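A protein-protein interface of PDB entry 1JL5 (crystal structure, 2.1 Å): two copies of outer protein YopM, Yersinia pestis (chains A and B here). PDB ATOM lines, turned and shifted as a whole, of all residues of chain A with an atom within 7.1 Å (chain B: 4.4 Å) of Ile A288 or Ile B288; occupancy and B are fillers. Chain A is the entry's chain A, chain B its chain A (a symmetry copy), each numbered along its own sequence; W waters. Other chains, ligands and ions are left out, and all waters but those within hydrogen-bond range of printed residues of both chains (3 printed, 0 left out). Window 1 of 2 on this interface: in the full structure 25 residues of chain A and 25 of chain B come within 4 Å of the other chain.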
ATOM      1  N   LYS A 250     -28.368 -13.609  20.790  1.00  0.00           N
ATOM      2  CA  LYS A 250     -27.483 -12.588  20.234  1.00  0.00           C
ATOM      3  C   LYS A 250     -27.761 -12.579  18.739  1.00  0.00           C
ATOM      4  O   LYS A 250     -27.507 -11.601  18.041  1.00  0.00           O
ATOM      5  CB  LYS A 250     -26.011 -12.943  20.463  1.00  0.00           C
ATOM      6  CG  LYS A 250     -25.634 -13.270  21.890  1.00  0.00           C
ATOM      7  CD  LYS A 250     -26.122 -14.661  22.269  1.00  0.00           C
ATOM      8  CE  LYS A 250     -25.709 -15.035  23.680  1.00  0.00           C
ATOM      9  NZ  LYS A 250     -26.292 -16.347  24.068  1.00  0.00           N
ATOM     10  N   ASN A 267     -33.819  -9.221  23.659  1.00  0.00           N
ATOM     11  CA  ASN A 267     -32.766 -10.174  23.437  1.00  0.00           C
ATOM     12  C   ASN A 267     -31.609  -9.289  23.083  1.00  0.00           C
ATOM     13  O   ASN A 267     -31.673  -8.085  23.291  1.00  0.00           O
ATOM     14  CB  ASN A 267     -33.127 -11.145  22.322  1.00  0.00           C
ATOM     15  CG  ASN A 267     -33.938 -12.309  22.838  1.00  0.00           C
ATOM     16  OD1 ASN A 267     -33.427 -13.137  23.593  1.00  0.00           O
ATOM     17  ND2 ASN A 267     -35.214 -12.369  22.459  1.00  0.00           N
ATOM     18  N   TYR A 268     -30.555  -9.856  22.541  1.00  0.00           N
ATOM     19  CA  TYR A 268     -29.407  -9.037  22.243  1.00  0.00           C
ATOM     20  C   TYR A 268     -29.186  -9.002  20.757  1.00  0.00           C
ATOM     21  O   TYR A 268     -28.056  -9.084  20.291  1.00  0.00           O
ATOM     22  CB  TYR A 268     -28.191  -9.619  22.944  1.00  0.00           C
ATOM     23  CG  TYR A 268     -27.162  -8.586  23.284  1.00  0.00           C
ATOM     24  CD1 TYR A 268     -27.440  -7.587  24.214  1.00  0.00           C
ATOM     25  CD2 TYR A 268     -25.900  -8.618  22.701  1.00  0.00           C
ATOM     26  CE1 TYR A 268     -26.480  -6.648  24.562  1.00  0.00           C
ATOM     27  CE2 TYR A 268     -24.936  -7.684  23.038  1.00  0.00           C
ATOM     28  CZ  TYR A 268     -25.233  -6.707  23.967  1.00  0.00           C
ATOM     29  OH  TYR A 268     -24.281  -5.789  24.301  1.00  0.00           O
ATOM     30  N   LEU A 269     -30.276  -8.871  20.016  1.00  0.00           N
ATOM     31  CA  LEU A 269     -30.195  -8.862  18.574  1.00  0.00           C
ATOM     32  C   LEU A 269     -29.822  -7.520  17.995  1.00  0.00           C
ATOM     33  O   LEU A 269     -30.401  -6.493  18.327  1.00  0.00           O
ATOM     34  CB  LEU A 269     -31.518  -9.318  17.980  1.00  0.00           C
ATOM     35  CG  LEU A 269     -31.955 -10.710  18.417  1.00  0.00           C
ATOM     36  CD1 LEU A 269     -33.323 -10.998  17.836  1.00  0.00           C
ATOM     37  CD2 LEU A 269     -30.933 -11.742  17.956  1.00  0.00           C
ATOM     38  N   THR A 270     -28.840  -7.546  17.114  1.00  0.00           N
ATOM     39  CA  THR A 270     -28.386  -6.347  16.444  1.00  0.00           C
ATOM     40  C   THR A 270     -28.826  -6.508  14.999  1.00  0.00           C
ATOM     41  O   THR A 270     -28.953  -5.548  14.245  1.00  0.00           O
ATOM     42  CB  THR A 270     -26.862  -6.245  16.482  1.00  0.00           C
ATOM     43  OG1 THR A 270     -26.457  -4.993  15.922  1.00  0.00           O
ATOM     44  CG2 THR A 270     -26.239  -7.369  15.673  1.00  0.00           C
ATOM     45  N   ASP A 271     -29.064  -7.754  14.627  1.00  0.00           N
ATOM     46  CA  ASP A 271     -29.466  -8.066  13.276  1.00  0.00           C
ATOM     47  C   ASP A 271     -30.461  -9.194  13.293  1.00  0.00           C
ATOM     48  O   ASP A 271     -30.618  -9.898  14.284  1.00  0.00           O
ATOM     49  CB  ASP A 271     -28.254  -8.495  12.441  1.00  0.00           C
ATOM     50  CG  ASP A 271     -27.224  -7.397  12.298  1.00  0.00           C
ATOM     51  OD1 ASP A 271     -27.564  -6.329  11.738  1.00  0.00           O
ATOM     52  OD2 ASP A 271     -26.073  -7.602  12.742  1.00  0.00           O
ATOM     53  N   VAL A 284     -39.156  -7.091  17.723  1.00  0.00           N
ATOM     54  CA  VAL A 284     -37.730  -7.129  17.980  1.00  0.00           C
ATOM     55  C   VAL A 284     -37.449  -6.011  18.958  1.00  0.00           C
ATOM     56  O   VAL A 284     -36.337  -5.505  19.046  1.00  0.00           O
ATOM     57  CB  VAL A 284     -36.933  -6.913  16.684  1.00  0.00           C
ATOM     58  CG1 VAL A 284     -37.154  -8.090  15.752  1.00  0.00           C
ATOM     59  CG2 VAL A 284     -37.371  -5.619  16.012  1.00  0.00           C
ATOM     60  N   SER A 285     -38.482  -5.623  19.695  1.00  0.00           N
ATOM     61  CA  SER A 285     -38.342  -4.555  20.660  1.00  0.00           C
ATOM     62  C   SER A 285     -37.339  -5.001  21.703  1.00  0.00           C
ATOM     63  O   SER A 285     -37.114  -6.196  21.903  1.00  0.00           O
ATOM     64  CB  SER A 285     -39.680  -4.257  21.329  1.00  0.00           C
ATOM     65  OG  SER A 285     -40.085  -5.345  22.130  1.00  0.00           O
ATOM     66  N   GLU A 286     -36.728  -4.028  22.355  1.00  0.00           N
ATOM     67  CA  GLU A 286     -35.750  -4.305  23.388  1.00  0.00           C
ATOM     68  C   GLU A 286     -34.626  -5.201  22.950  1.00  0.00           C
ATOM     69  O   GLU A 286     -34.264  -6.150  23.631  1.00  0.00           O
ATOM     70  CB  GLU A 286     -36.413  -4.909  24.611  1.00  0.00           C
ATOM     71  CG  GLU A 286     -37.099  -3.882  25.470  1.00  0.00           C
ATOM     72  CD  GLU A 286     -37.612  -4.493  26.743  1.00  0.00           C
ATOM     73  OE1 GLU A 286     -36.801  -5.043  27.513  1.00  0.00           O
ATOM     74  OE2 GLU A 286     -38.828  -4.433  26.971  1.00  0.00           O
ATOM     75  N   ASN A 287     -34.096  -4.921  21.779  1.00  0.00           N
ATOM     76  CA  ASN A 287     -32.950  -5.655  21.331  1.00  0.00           C
ATOM     77  C   ASN A 287     -31.947  -4.561  21.143  1.00  0.00           C
ATOM     78  O   ASN A 287     -32.083  -3.501  21.751  1.00  0.00           O
ATOM     79  CB  ASN A 287     -33.263  -6.418  20.060  1.00  0.00           C
ATOM     80  CG  ASN A 287     -33.833  -7.771  20.365  1.00  0.00           C
ATOM     81  OD1 ASN A 287     -33.094  -8.700  20.665  1.00  0.00           O
ATOM     82  ND2 ASN A 287     -35.154  -7.884  20.340  1.00  0.00           N
ATOM     83  N   ILE A 288     -30.944  -4.773  20.319  1.00  0.00           N
ATOM     84  CA  ILE A 288     -29.969  -3.721  20.174  1.00  0.00           C
ATOM     85  C   ILE A 288     -29.805  -3.330  18.734  1.00  0.00           C
ATOM     86  O   ILE A 288     -28.702  -3.135  18.238  1.00  0.00           O
ATOM     87  CB  ILE A 288     -28.639  -4.137  20.814  1.00  0.00           C
ATOM     88  CG1 ILE A 288     -28.080  -5.392  20.146  1.00  0.00           C
ATOM     89  CG2 ILE A 288     -28.878  -4.441  22.284  1.00  0.00           C
ATOM     90  CD1 ILE A 288     -26.706  -5.784  20.679  1.00  0.00           C
ATOM     91  N   PHE A 289     -30.940  -3.220  18.062  1.00  0.00           N
ATOM     92  CA  PHE A 289     -30.957  -2.820  16.673  1.00  0.00           C
ATOM     93  C   PHE A 289     -30.661  -1.340  16.614  1.00  0.00           C
ATOM     94  O   PHE A 289     -31.260  -0.552  17.343  1.00  0.00           O
ATOM     95  CB  PHE A 289     -32.330  -3.090  16.072  1.00  0.00           C
ATOM     96  CG  PHE A 289     -32.605  -4.534  15.862  1.00  0.00           C
ATOM     97  CD1 PHE A 289     -32.100  -5.192  14.749  1.00  0.00           C
ATOM     98  CD2 PHE A 289     -33.340  -5.255  16.795  1.00  0.00           C
ATOM     99  CE1 PHE A 289     -32.318  -6.552  14.573  1.00  0.00           C
ATOM    100  CE2 PHE A 289     -33.560  -6.611  16.626  1.00  0.00           C
ATOM    101  CZ  PHE A 289     -33.049  -7.260  15.511  1.00  0.00           C
ATOM    102  N   SER A 290     -29.718  -0.966  15.766  1.00  0.00           N
ATOM    103  CA  SER A 290     -29.378   0.439  15.602  1.00  0.00           C
ATOM    104  C   SER A 290     -30.238   0.912  14.440  1.00  0.00           C
ATOM    105  O   SER A 290     -30.304   2.095  14.118  1.00  0.00           O
ATOM    106  CB  SER A 290     -27.893   0.594  15.286  1.00  0.00           C
ATOM    107  OG  SER A 290     -27.529  -0.252  14.218  1.00  0.00           O
ATOM    108  N   GLY A 291     -30.914  -0.045  13.824  1.00  0.00           N
ATOM    109  CA  GLY A 291     -31.794   0.260  12.721  1.00  0.00           C
ATOM    110  C   GLY A 291     -32.414  -1.015  12.196  1.00  0.00           C
ATOM    111  O   GLY A 291     -32.094  -2.109  12.648  1.00  0.00           O
ATOM    112  N   SER A 306     -37.772   0.409  21.888  1.00  0.00           N
ATOM    113  CA  SER A 306     -36.676   0.219  22.819  1.00  0.00           C
ATOM    114  C   SER A 306     -35.475  -0.511  22.263  1.00  0.00           C
ATOM    115  O   SER A 306     -34.933  -1.425  22.875  1.00  0.00           O
ATOM    116  CB  SER A 306     -37.193  -0.479  24.069  1.00  0.00           C
ATOM    117  OG  SER A 306     -38.052   0.415  24.751  1.00  0.00           O
ATOM    118  N   ASN A 307     -35.082  -0.103  21.072  1.00  0.00           N
ATOM    119  CA  ASN A 307     -33.901  -0.637  20.444  1.00  0.00           C
ATOM    120  C   ASN A 307     -33.080   0.617  20.382  1.00  0.00           C
ATOM    121  O   ASN A 307     -33.252   1.502  21.208  1.00  0.00           O
ATOM    122  CB  ASN A 307     -34.223  -1.167  19.052  1.00  0.00           C
ATOM    123  CG  ASN A 307     -34.624  -2.617  19.086  1.00  0.00           C
ATOM    124  OD1 ASN A 307     -33.785  -3.486  19.296  1.00  0.00           O
ATOM    125  ND2 ASN A 307     -35.915  -2.891  18.914  1.00  0.00           N
ATOM    126  N   GLU A 308     -32.186   0.710  19.423  1.00  0.00           N
ATOM    127  CA  GLU A 308     -31.402   1.917  19.302  1.00  0.00           C
ATOM    128  C   GLU A 308     -31.574   2.304  17.849  1.00  0.00           C
ATOM    129  O   GLU A 308     -30.653   2.778  17.197  1.00  0.00           O
ATOM    130  CB  GLU A 308     -29.939   1.638  19.638  1.00  0.00           C
ATOM    131  CG  GLU A 308     -29.155   2.901  19.888  1.00  0.00           C
ATOM    132  CD  GLU A 308     -29.564   3.591  21.170  1.00  0.00           C
ATOM    133  OE1 GLU A 308     -30.672   3.320  21.689  1.00  0.00           O
ATOM    134  OE2 GLU A 308     -28.772   4.415  21.661  1.00  0.00           O
ATOM    135  N   ILE A 309     -32.785   2.077  17.352  1.00  0.00           N
ATOM    136  CA  ILE A 309     -33.106   2.361  15.966  1.00  0.00           C
ATOM    137  C   ILE A 309     -32.914   3.825  15.648  1.00  0.00           C
ATOM    138  O   ILE A 309     -33.615   4.687  16.173  1.00  0.00           O
ATOM    139  CB  ILE A 309     -34.558   1.998  15.628  1.00  0.00           C
ATOM    140  CG1 ILE A 309     -34.827   0.523  15.957  1.00  0.00           C
ATOM    141  CG2 ILE A 309     -34.825   2.285  14.159  1.00  0.00           C
ATOM    142  CD1 ILE A 309     -33.901  -0.414  15.278  1.00  0.00           C
ATOM    143  N   TYR B 268     -26.038   3.161  23.602  1.00  0.00           N
ATOM    144  CA  TYR B 268     -25.655   1.879  23.068  1.00  0.00           C
ATOM    145  C   TYR B 268     -24.408   1.399  23.755  1.00  0.00           C
ATOM    146  O   TYR B 268     -23.507   0.867  23.118  1.00  0.00           O
ATOM    147  CB  TYR B 268     -25.413   2.019  21.574  1.00  0.00           C
ATOM    148  CG  TYR B 268     -25.676   0.754  20.817  1.00  0.00           C
ATOM    149  CD1 TYR B 268     -26.963   0.229  20.739  1.00  0.00           C
ATOM    150  CD2 TYR B 268     -24.647   0.093  20.156  1.00  0.00           C
ATOM    151  CE1 TYR B 268     -27.222  -0.922  20.010  1.00  0.00           C
ATOM    152  CE2 TYR B 268     -24.893  -1.058  19.428  1.00  0.00           C
ATOM    153  CZ  TYR B 268     -26.179  -1.557  19.360  1.00  0.00           C
ATOM    154  OH  TYR B 268     -26.421  -2.689  18.639  1.00  0.00           O
ATOM    155  N   LEU B 269     -24.365   1.586  25.066  1.00  0.00           N
ATOM    156  CA  LEU B 269     -23.203   1.200  25.833  1.00  0.00           C
ATOM    157  C   LEU B 269     -23.170  -0.264  26.191  1.00  0.00           C
ATOM    158  O   LEU B 269     -24.134  -0.824  26.698  1.00  0.00           O
ATOM    159  CB  LEU B 269     -23.123   2.032  27.103  1.00  0.00           C
ATOM    160  CG  LEU B 269     -23.051   3.535  26.864  1.00  0.00           C
ATOM    161  CD1 LEU B 269     -23.074   4.244  28.202  1.00  0.00           C
ATOM    162  CD2 LEU B 269     -21.787   3.875  26.083  1.00  0.00           C
ATOM    163  N   THR B 270     -22.034  -0.880  25.921  1.00  0.00           N
ATOM    164  CA  THR B 270     -21.831  -2.278  26.234  1.00  0.00           C
ATOM    165  C   THR B 270     -20.823  -2.288  27.369  1.00  0.00           C
ATOM    166  O   THR B 270     -20.708  -3.246  28.129  1.00  0.00           O
ATOM    167  CB  THR B 270     -21.233  -3.022  25.041  1.00  0.00           C
ATOM    168  OG1 THR B 270     -21.161  -4.418  25.342  1.00  0.00           O
ATOM    169  CG2 THR B 270     -19.833  -2.510  24.751  1.00  0.00           C
ATOM    170  N   ASN B 287     -29.158   0.242  27.986  1.00  0.00           N
ATOM    171  CA  ASN B 287     -27.981   0.273  27.171  1.00  0.00           C
ATOM    172  C   ASN B 287     -27.868  -1.158  26.752  1.00  0.00           C
ATOM    173  O   ASN B 287     -28.867  -1.875  26.761  1.00  0.00           O
ATOM    174  CB  ASN B 287     -26.789   0.770  27.965  1.00  0.00           C
ATOM    175  CG  ASN B 287     -26.690   2.265  27.915  1.00  0.00           C
ATOM    176  OD1 ASN B 287     -26.193   2.820  26.943  1.00  0.00           O
ATOM    177  ND2 ASN B 287     -27.205   2.934  28.939  1.00  0.00           N
ATOM    178  N   ILE B 288     -26.686  -1.608  26.388  1.00  0.00           N
ATOM    179  CA  ILE B 288     -26.601  -2.981  25.958  1.00  0.00           C
ATOM    180  C   ILE B 288     -25.570  -3.734  26.747  1.00  0.00           C
ATOM    181  O   ILE B 288     -24.779  -4.501  26.214  1.00  0.00           O
ATOM    182  CB  ILE B 288     -26.333  -3.049  24.449  1.00  0.00           C
ATOM    183  CG1 ILE B 288     -25.015  -2.362  24.096  1.00  0.00           C
ATOM    184  CG2 ILE B 288     -27.459  -2.331  23.721  1.00  0.00           C
ATOM    185  CD1 ILE B 288     -24.655  -2.495  22.620  1.00  0.00           C
ATOM    186  N   PHE B 289     -25.593  -3.493  28.048  1.00  0.00           N
ATOM    187  CA  PHE B 289     -24.686  -4.162  28.954  1.00  0.00           C
ATOM    188  C   PHE B 289     -25.155  -5.590  29.107  1.00  0.00           C
ATOM    189  O   PHE B 289     -26.335  -5.840  29.346  1.00  0.00           O
ATOM    190  CB  PHE B 289     -24.704  -3.471  30.311  1.00  0.00           C
ATOM    191  CG  PHE B 289     -24.031  -2.147  30.305  1.00  0.00           C
ATOM    192  CD1 PHE B 289     -22.648  -2.061  30.391  1.00  0.00           C
ATOM    193  CD2 PHE B 289     -24.772  -0.980  30.174  1.00  0.00           C
ATOM    194  CE1 PHE B 289     -22.012  -0.828  30.341  1.00  0.00           C
ATOM    195  CE2 PHE B 289     -24.146   0.253  30.122  1.00  0.00           C
ATOM    196  CZ  PHE B 289     -22.762   0.329  30.207  1.00  0.00           C
ATOM    197  N   SER B 290     -24.237  -6.528  28.943  1.00  0.00           N
ATOM    198  CA  SER B 290     -24.571  -7.934  29.105  1.00  0.00           C
ATOM    199  C   SER B 290     -24.246  -8.245  30.558  1.00  0.00           C
ATOM    200  O   SER B 290     -24.540  -9.319  31.075  1.00  0.00           O
ATOM    201  CB  SER B 290     -23.735  -8.791  28.159  1.00  0.00           C
ATOM    202  OG  SER B 290     -22.368  -8.470  28.285  1.00  0.00           O
ATOM    203  N   ASN B 307     -31.143  -3.677  30.308  1.00  0.00           N
ATOM    204  CA  ASN B 307     -29.896  -3.877  29.616  1.00  0.00           C
ATOM    205  C   ASN B 307     -30.031  -5.339  29.305  1.00  0.00           C
ATOM    206  O   ASN B 307     -31.141  -5.836  29.176  1.00  0.00           O
ATOM    207  CB  ASN B 307     -28.715  -3.607  30.541  1.00  0.00           C
ATOM    208  CG  ASN B 307     -28.286  -2.166  30.492  1.00  0.00           C
ATOM    209  OD1 ASN B 307     -27.701  -1.728  29.508  1.00  0.00           O
ATOM    210  ND2 ASN B 307     -28.602  -1.406  31.538  1.00  0.00           N
HETATM  211  O   HOH W   1     -21.852  -7.624  25.203  1.00  0.00           O
HETATM  212  O   HOH W   2     -25.254  -1.942  15.783  1.00  0.00           O
HETATM  213  O   HOH W   3     -26.544   4.771  20.607  1.00  0.00           O
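The side-chain hydroxyl (OH) of Tyr A268 lies close to the backbone carbonyl oxygen (O) of Ile B288, 2.4 Å away.
The side-chain hydroxyl of Tyr B268 lies close to the backbone carbonyl oxygen of Ile A288.
Among the printed residues, merely in contact across the chains: Tyr A268 with Thr B270 (3.6 Å), Thr A270 with Tyr B268 (3.6 Å), Ile A288 with Ile B288 (2.9 Å) and Glu A308 with Tyr B268 (3.5 Å).
Tyr A268 touches Thr B270, and with the chains exchanged Thr A270 touches Tyr B268.
Tyr A268 touches Ile B288, and with the chains exchanged Ile A288 touches Tyr B268.
Ile A288 touches its own counterpart, Ile B288.
Positions printed for both chains: 268, 269, 270, 287, 288, 289, 290 and 307.
Of the 6 pairs that touch across the chains among the printed residues, 5 have their exchanged pair printed and touching as well.
Of the 18 printed residues of chain A, 4 touch a printed residue of chain B.
Hydrophobic or aromatic side chains of chain A within 4 Å of the printed part of chain B: Tyr A268 and Ile A288.
Water W3 bridges the side-chain carboxylate (OE2) of Glu A308 and the backbone NH (N) of Tyr B268.
Water W2 lies within hydrogen-bond range of the side-chain hydroxyl of Tyr B268, the side-chain hydroxyl of Ser A290 and the side-chain hydroxyl of Thr A270.
Water W1 lies within hydrogen-bond range of the side-chain hydroxyl of Tyr A268, the side-chain hydroxyl of Ser B290 and the side-chain hydroxyl of Thr B270.
Of the printed residues of chain B, Tyr A268 touches Thr B270 (3.6 Å) and Ile B288 (2.4 Å).
Printed residues of chain B within 4 Å of Thr A270: Tyr B268.
Ile A288 touches two residues of chain B.
Ile B288 touches two residues of chain A.
The backbone NH of Tyr A268 lies within hydrogen-bond range of the side-chain amide oxygen of Asn A287 (3.4 Å).
The backbone carbonyl oxygen (O) of Leu A269 lies within hydrogen-bond range of the backbone NH (N) of Ile A288.
The backbone NH (N) of Ile A288 is in hydrogen-bond range of the side-chain amide oxygen (OD1) of Asn A307.
The backbone carbonyl oxygen (O) of Phe A289 is in hydrogen-bond range of the backbone NH (N) of Glu A308, at 2.6 Å.
The side-chain amide oxygen (OD1) of Asn B287 is in hydrogen-bond range of the backbone NH (N) of Tyr B268 (3.4 Å).
The backbone carbonyl oxygen of Leu B269 lies within hydrogen-bond range of the backbone NH of Ile B288 (2.7 Å).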
